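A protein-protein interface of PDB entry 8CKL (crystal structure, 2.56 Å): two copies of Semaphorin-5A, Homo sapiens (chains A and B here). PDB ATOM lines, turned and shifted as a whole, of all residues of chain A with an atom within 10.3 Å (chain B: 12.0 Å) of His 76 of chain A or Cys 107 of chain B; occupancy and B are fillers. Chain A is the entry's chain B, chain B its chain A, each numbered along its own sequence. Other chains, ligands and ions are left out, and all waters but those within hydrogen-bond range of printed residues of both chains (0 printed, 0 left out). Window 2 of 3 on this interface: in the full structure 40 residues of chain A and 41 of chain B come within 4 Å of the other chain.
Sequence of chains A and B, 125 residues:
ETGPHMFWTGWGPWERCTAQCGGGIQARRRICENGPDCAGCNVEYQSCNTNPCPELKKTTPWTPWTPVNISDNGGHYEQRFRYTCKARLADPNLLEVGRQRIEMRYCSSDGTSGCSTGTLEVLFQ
Hydrophobic or aromatic side chains of chain B that line the printed part of chain A: Met 104 and Tyr 106. Hydrophobic or aromatic side chains of chain A within 4 Å of the printed part of chain B: Trp 65, His 76 and Tyr 77.
Thr 66 of chain A touches its own counterpart, Thr 66 of chain B. 3 positions are printed for both chains. Of the 11 pairs that touch across the chains among the printed residues, 1 has its exchanged pair printed and touching as well.
Of the printed residues of chain B, Trp 65 of chain A touches Glu 103 and Arg 105. Of the printed residues of chain B, Thr 66 of chain A touches Thr 66. His 76 of chain A touches just these residues of chain B: Tyr 106 (3.2 Å) and Cys 107 (2.7 Å). Of the printed residues of chain B, Gln 79 of chain A touches Glu 103. Of the printed residues of chain A, Thr 66 of chain B touches Thr 66 (3.5 Å). Val 68 of chain B touches none of the printed residues of chain A. Of the printed residues of chain A, Arg 105 of chain B touches Trp 65, Tyr 77 and Glu 78. Tyr 106 of chain B touches two residues of chain A. Cys 107 of chain B touches just these residues of chain A: His 76 (2.7 Å) and Glu 78 (3.5 Å). No residue of chain A comes within 4 Å of Ser 108 of chain B. The nearest residue of chain B that does not touch His 76 of chain A is Arg 105 of chain B (4.5 Å). The nearest residue of chain A that does not touch Cys 107 of chain B is Tyr 77 of chain A (4.8 Å). The nearest printed residue of chain B that does not touch Glu 78 of chain A is Glu 103 of chain B (4.01 Å).
Among the printed residues, merely in contact across the chains: Trp 65 of chain A with Glu 103 of chain B (3.6 Å), Trp 65 of chain A with Arg 105 of chain B (3.2 Å), Thr 66 of chain A with Thr 66 of chain B (3.5 Å), His 76 of chain A with Tyr 106 of chain B (3.2 Å), Tyr 77 of chain A with Arg 105 of chain B (3.4 Å), Tyr 77 of chain A with Tyr 106 of chain B (3.5 Å), Glu 78 of chain A with Met 104 of chain B (3.3 Å) and Gln 79 of chain A with Glu 103 of chain B (3.2 Å).
The backbone NH (N) of Val 68 of chain A is in hydrogen-bond range of the backbone carbonyl oxygen (O) of Tyr 77 of chain A (3.1 Å). O of Thr 66 of chain A sits at hydrogen-bond distance from N of Gln 79 of chain A.
NH2 of Arg 105 of chain B lies within salt-bridge range of OE1 of Glu 78 of chain A (2.7 Å). The backbone carbonyl oxygen (O) of Cys 107 of chain B sits at hydrogen-bond distance from the backbone NH (N) of His 76 of chain A (2.7 Å). The side-chain sulfur of Cys 107 of chain B lies within hydrogen-bond range of the side-chain carboxylate of Glu 78 of chain A, 3.5 Å away.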
ATOM      1  N   TRP A  65     -11.942  -4.252 -28.976  1.00  0.00           N
ATOM      2  CA  TRP A  65     -12.234  -5.666 -28.776  1.00  0.00           C
ATOM      3  C   TRP A  65     -12.035  -6.433 -30.078  1.00  0.00           C
ATOM      4  O   TRP A  65     -12.568  -6.052 -31.124  1.00  0.00           O
ATOM      5  CB  TRP A  65     -13.667  -5.854 -28.274  1.00  0.00           C
ATOM      6  CG  TRP A  65     -13.912  -5.360 -26.878  1.00  0.00           C
ATOM      7  CD1 TRP A  65     -14.435  -4.153 -26.516  1.00  0.00           C
ATOM      8  CD2 TRP A  65     -13.653  -6.065 -25.658  1.00  0.00           C
ATOM      9  NE1 TRP A  65     -14.516  -4.062 -25.148  1.00  0.00           N
ATOM     10  CE2 TRP A  65     -14.042  -5.223 -24.597  1.00  0.00           C
ATOM     11  CE3 TRP A  65     -13.128  -7.326 -25.359  1.00  0.00           C
ATOM     12  CZ2 TRP A  65     -13.922  -5.601 -23.261  1.00  0.00           C
ATOM     13  CZ3 TRP A  65     -13.009  -7.698 -24.031  1.00  0.00           C
ATOM     14  CH2 TRP A  65     -13.404  -6.839 -23.000  1.00  0.00           C
ATOM     15  N   THR A  66     -11.261  -7.513 -30.010  1.00  0.00           N
ATOM     16  CA  THR A  66     -10.992  -8.340 -31.173  1.00  0.00           C
ATOM     17  C   THR A  66     -11.295  -9.797 -30.856  1.00  0.00           C
ATOM     18  O   THR A  66     -11.077 -10.246 -29.723  1.00  0.00           O
ATOM     19  CB  THR A  66      -9.527  -8.207 -31.624  1.00  0.00           C
ATOM     20  OG1 THR A  66      -8.658  -8.592 -30.553  1.00  0.00           O
ATOM     21  CG2 THR A  66      -9.219  -6.775 -32.037  1.00  0.00           C
ATOM     22  N   PRO A  67     -11.799 -10.557 -31.825  1.00  0.00           N
ATOM     23  CA  PRO A  67     -12.052 -11.981 -31.586  1.00  0.00           C
ATOM     24  C   PRO A  67     -10.756 -12.751 -31.397  1.00  0.00           C
ATOM     25  O   PRO A  67      -9.698 -12.375 -31.909  1.00  0.00           O
ATOM     26  CB  PRO A  67     -12.787 -12.429 -32.855  1.00  0.00           C
ATOM     27  CG  PRO A  67     -12.352 -11.458 -33.900  1.00  0.00           C
ATOM     28  CD  PRO A  67     -12.181 -10.147 -33.188  1.00  0.00           C
ATOM     29  N   VAL A  68     -10.850 -13.843 -30.647  1.00  0.00           N
ATOM     30  CA  VAL A  68      -9.691 -14.683 -30.374  1.00  0.00           C
ATOM     31  C   VAL A  68      -9.469 -15.665 -31.519  1.00  0.00           C
ATOM     32  O   VAL A  68      -8.662 -15.416 -32.415  1.00  0.00           O
ATOM     33  CB  VAL A  68      -9.847 -15.431 -29.039  1.00  0.00           C
ATOM     34  CG1 VAL A  68      -8.597 -16.244 -28.739  1.00  0.00           C
ATOM     35  CG2 VAL A  68     -10.135 -14.451 -27.914  1.00  0.00           C
ATOM     36  N   HIS A  76     -18.583 -16.350 -29.686  1.00  0.00           N
ATOM     37  CA  HIS A  76     -17.127 -16.398 -29.655  1.00  0.00           C
ATOM     38  C   HIS A  76     -16.614 -15.524 -28.512  1.00  0.00           C
ATOM     39  O   HIS A  76     -17.391 -14.851 -27.834  1.00  0.00           O
ATOM     40  CB  HIS A  76     -16.527 -15.933 -30.983  1.00  0.00           C
ATOM     41  CG  HIS A  76     -16.695 -14.468 -31.240  1.00  0.00           C
ATOM     42  ND1 HIS A  76     -17.888 -13.902 -31.638  1.00  0.00           N
ATOM     43  CD2 HIS A  76     -15.815 -13.445 -31.128  1.00  0.00           C
ATOM     44  CE1 HIS A  76     -17.731 -12.597 -31.776  1.00  0.00           C
ATOM     45  NE2 HIS A  76     -16.482 -12.293 -31.470  1.00  0.00           N
ATOM     46  N   TYR A  77     -15.306 -15.539 -28.290  1.00  0.00           N
ATOM     47  CA  TYR A  77     -14.691 -14.754 -27.231  1.00  0.00           C
ATOM     48  C   TYR A  77     -13.983 -13.542 -27.819  1.00  0.00           C
ATOM     49  O   TYR A  77     -13.452 -13.584 -28.934  1.00  0.00           O
ATOM     50  CB  TYR A  77     -13.700 -15.592 -26.419  1.00  0.00           C
ATOM     51  CG  TYR A  77     -14.354 -16.570 -25.472  1.00  0.00           C
ATOM     52  CD1 TYR A  77     -14.649 -17.865 -25.875  1.00  0.00           C
ATOM     53  CD2 TYR A  77     -14.676 -16.199 -24.172  1.00  0.00           C
ATOM     54  CE1 TYR A  77     -15.245 -18.764 -25.010  1.00  0.00           C
ATOM     55  CE2 TYR A  77     -15.271 -17.089 -23.301  1.00  0.00           C
ATOM     56  CZ  TYR A  77     -15.553 -18.369 -23.726  1.00  0.00           C
ATOM     57  OH  TYR A  77     -16.147 -19.259 -22.860  1.00  0.00           O
ATOM     58  N   GLU A  78     -13.993 -12.456 -27.053  1.00  0.00           N
ATOM     59  CA  GLU A  78     -13.343 -11.212 -27.431  1.00  0.00           C
ATOM     60  C   GLU A  78     -12.301 -10.855 -26.384  1.00  0.00           C
ATOM     61  O   GLU A  78     -12.494 -11.106 -25.190  1.00  0.00           O
ATOM     62  CB  GLU A  78     -14.352 -10.065 -27.566  1.00  0.00           C
ATOM     63  CG  GLU A  78     -15.217 -10.122 -28.813  1.00  0.00           C
ATOM     64  CD  GLU A  78     -16.126  -8.913 -28.943  1.00  0.00           C
ATOM     65  OE1 GLU A  78     -16.189  -8.107 -27.989  1.00  0.00           O
ATOM     66  OE2 GLU A  78     -16.774  -8.765 -30.000  1.00  0.00           O
ATOM     67  N   GLN A  79     -11.196 -10.267 -26.836  1.00  0.00           N
ATOM     68  CA  GLN A  79     -10.106  -9.892 -25.951  1.00  0.00           C
ATOM     69  C   GLN A  79      -9.575  -8.524 -26.351  1.00  0.00           C
ATOM     70  O   GLN A  79      -9.658  -8.123 -27.515  1.00  0.00           O
ATOM     71  CB  GLN A  79      -8.969 -10.921 -25.993  1.00  0.00           C
ATOM     72  CG  GLN A  79      -8.323 -11.060 -27.364  1.00  0.00           C
ATOM     73  CD  GLN A  79      -7.236 -12.115 -27.400  1.00  0.00           C
ATOM     74  OE1 GLN A  79      -6.965 -12.780 -26.398  1.00  0.00           O
ATOM     75  NE2 GLN A  79      -6.604 -12.272 -28.557  1.00  0.00           N
ATOM     76  N   THR B  66      -4.125  -9.784 -34.188  1.00  0.00           N
ATOM     77  CA  THR B  66      -5.506 -10.224 -34.107  1.00  0.00           C
ATOM     78  C   THR B  66      -6.216  -9.936 -35.422  1.00  0.00           C
ATOM     79  O   THR B  66      -5.936  -8.919 -36.070  1.00  0.00           O
ATOM     80  CB  THR B  66      -6.251  -9.527 -32.957  1.00  0.00           C
ATOM     81  OG1 THR B  66      -6.216  -8.107 -33.152  1.00  0.00           O
ATOM     82  CG2 THR B  66      -5.615  -9.867 -31.617  1.00  0.00           C
ATOM     83  N   PRO B  67      -7.129 -10.807 -35.844  1.00  0.00           N
ATOM     84  CA  PRO B  67      -7.888 -10.537 -37.069  1.00  0.00           C
ATOM     85  C   PRO B  67      -8.826  -9.355 -36.889  1.00  0.00           C
ATOM     86  O   PRO B  67      -9.282  -9.053 -35.783  1.00  0.00           O
ATOM     87  CB  PRO B  67      -8.665 -11.838 -37.300  1.00  0.00           C
ATOM     88  CG  PRO B  67      -8.772 -12.454 -35.944  1.00  0.00           C
ATOM     89  CD  PRO B  67      -7.496 -12.097 -35.237  1.00  0.00           C
ATOM     90  N   VAL B  68      -9.109  -8.680 -37.998  1.00  0.00           N
ATOM     91  CA  VAL B  68      -9.997  -7.524 -37.978  1.00  0.00           C
ATOM     92  C   VAL B  68     -11.450  -7.976 -38.062  1.00  0.00           C
ATOM     93  O   VAL B  68     -11.955  -8.277 -39.144  1.00  0.00           O
ATOM     94  CB  VAL B  68      -9.666  -6.546 -39.116  1.00  0.00           C
ATOM     95  CG1 VAL B  68     -10.555  -5.315 -39.032  1.00  0.00           C
ATOM     96  CG2 VAL B  68      -8.198  -6.153 -39.066  1.00  0.00           C
ATOM     97  N   GLU B 103      -7.890  -8.312 -21.095  1.00  0.00           N
ATOM     98  CA  GLU B 103      -9.264  -8.479 -20.644  1.00  0.00           C
ATOM     99  C   GLU B 103     -10.050  -9.290 -21.663  1.00  0.00           C
ATOM    100  O   GLU B 103      -9.929  -9.068 -22.871  1.00  0.00           O
ATOM    101  CB  GLU B 103      -9.935  -7.123 -20.424  1.00  0.00           C
ATOM    102  CG  GLU B 103     -11.349  -7.211 -19.888  1.00  0.00           C
ATOM    103  CD  GLU B 103     -11.973  -5.849 -19.681  1.00  0.00           C
ATOM    104  OE1 GLU B 103     -11.580  -4.897 -20.388  1.00  0.00           O
ATOM    105  OE2 GLU B 103     -12.854  -5.729 -18.807  1.00  0.00           O
ATOM    106  N   MET B 104     -10.859 -10.229 -21.175  1.00  0.00           N
ATOM    107  CA  MET B 104     -11.605 -11.137 -22.034  1.00  0.00           C
ATOM    108  C   MET B 104     -13.082 -11.122 -21.669  1.00  0.00           C
ATOM    109  O   MET B 104     -13.454 -10.895 -20.515  1.00  0.00           O
ATOM    110  CB  MET B 104     -11.064 -12.571 -21.939  1.00  0.00           C
ATOM    111  CG  MET B 104      -9.612 -12.716 -22.363  1.00  0.00           C
ATOM    112  SD  MET B 104      -8.994 -14.394 -22.148  1.00  0.00           S
ATOM    113  CE  MET B 104     -10.133 -15.306 -23.188  1.00  0.00           C
ATOM    114  N   ARG B 105     -13.920 -11.365 -22.675  1.00  0.00           N
ATOM    115  CA  ARG B 105     -15.362 -11.455 -22.499  1.00  0.00           C
ATOM    116  C   ARG B 105     -15.920 -12.344 -23.599  1.00  0.00           C
ATOM    117  O   ARG B 105     -15.261 -12.595 -24.612  1.00  0.00           O
ATOM    118  CB  ARG B 105     -16.041 -10.082 -22.545  1.00  0.00           C
ATOM    119  CG  ARG B 105     -16.018  -9.439 -23.923  1.00  0.00           C
ATOM    120  CD  ARG B 105     -16.697  -8.079 -23.926  1.00  0.00           C
ATOM    121  NE  ARG B 105     -16.693  -7.481 -25.256  1.00  0.00           N
ATOM    122  CZ  ARG B 105     -17.191  -6.286 -25.544  1.00  0.00           C
ATOM    123  NH1 ARG B 105     -17.745  -5.525 -24.614  1.00  0.00           N
ATOM    124  NH2 ARG B 105     -17.133  -5.845 -26.797  1.00  0.00           N
ATOM    125  N   TYR B 106     -17.144 -12.820 -23.394  1.00  0.00           N
ATOM    126  CA  TYR B 106     -17.804 -13.697 -24.348  1.00  0.00           C
ATOM    127  C   TYR B 106     -18.980 -12.982 -24.998  1.00  0.00           C
ATOM    128  O   TYR B 106     -19.768 -12.315 -24.319  1.00  0.00           O
ATOM    129  CB  TYR B 106     -18.291 -14.984 -23.678  1.00  0.00           C
ATOM    130  CG  TYR B 106     -18.973 -15.936 -24.635  1.00  0.00           C
ATOM    131  CD1 TYR B 106     -18.234 -16.824 -25.406  1.00  0.00           C
ATOM    132  CD2 TYR B 106     -20.357 -15.941 -24.774  1.00  0.00           C
ATOM    133  CE1 TYR B 106     -18.851 -17.692 -26.285  1.00  0.00           C
ATOM    134  CE2 TYR B 106     -20.983 -16.807 -25.651  1.00  0.00           C
ATOM    135  CZ  TYR B 106     -20.226 -17.680 -26.402  1.00  0.00           C
ATOM    136  OH  TYR B 106     -20.845 -18.543 -27.277  1.00  0.00           O
ATOM    137  N   CYS B 107     -19.093 -13.129 -26.315  1.00  0.00           N
ATOM    138  CA  CYS B 107     -20.192 -12.567 -27.087  1.00  0.00           C
ATOM    139  C   CYS B 107     -20.864 -13.677 -27.880  1.00  0.00           C
ATOM    140  O   CYS B 107     -20.188 -14.529 -28.464  1.00  0.00           O
ATOM    141  CB  CYS B 107     -19.705 -11.461 -28.031  1.00  0.00           C
ATOM    142  SG  CYS B 107     -19.008 -10.019 -27.192  1.00  0.00           S
ATOM    143  N   SER B 108     -22.192 -13.666 -27.898  1.00  0.00           N
ATOM    144  CA  SER B 108     -22.952 -14.676 -28.626  1.00  0.00           C
ATOM    145  C   SER B 108     -23.697 -14.059 -29.805  1.00  0.00           C
ATOM    146  O   SER B 108     -23.240 -13.083 -30.400  1.00  0.00           O
ATOM    147  CB  SER B 108     -23.937 -15.383 -27.694  1.00  0.00           C
ATOM    148  OG  SER B 108     -24.879 -14.471 -27.162  1.00  0.00           O
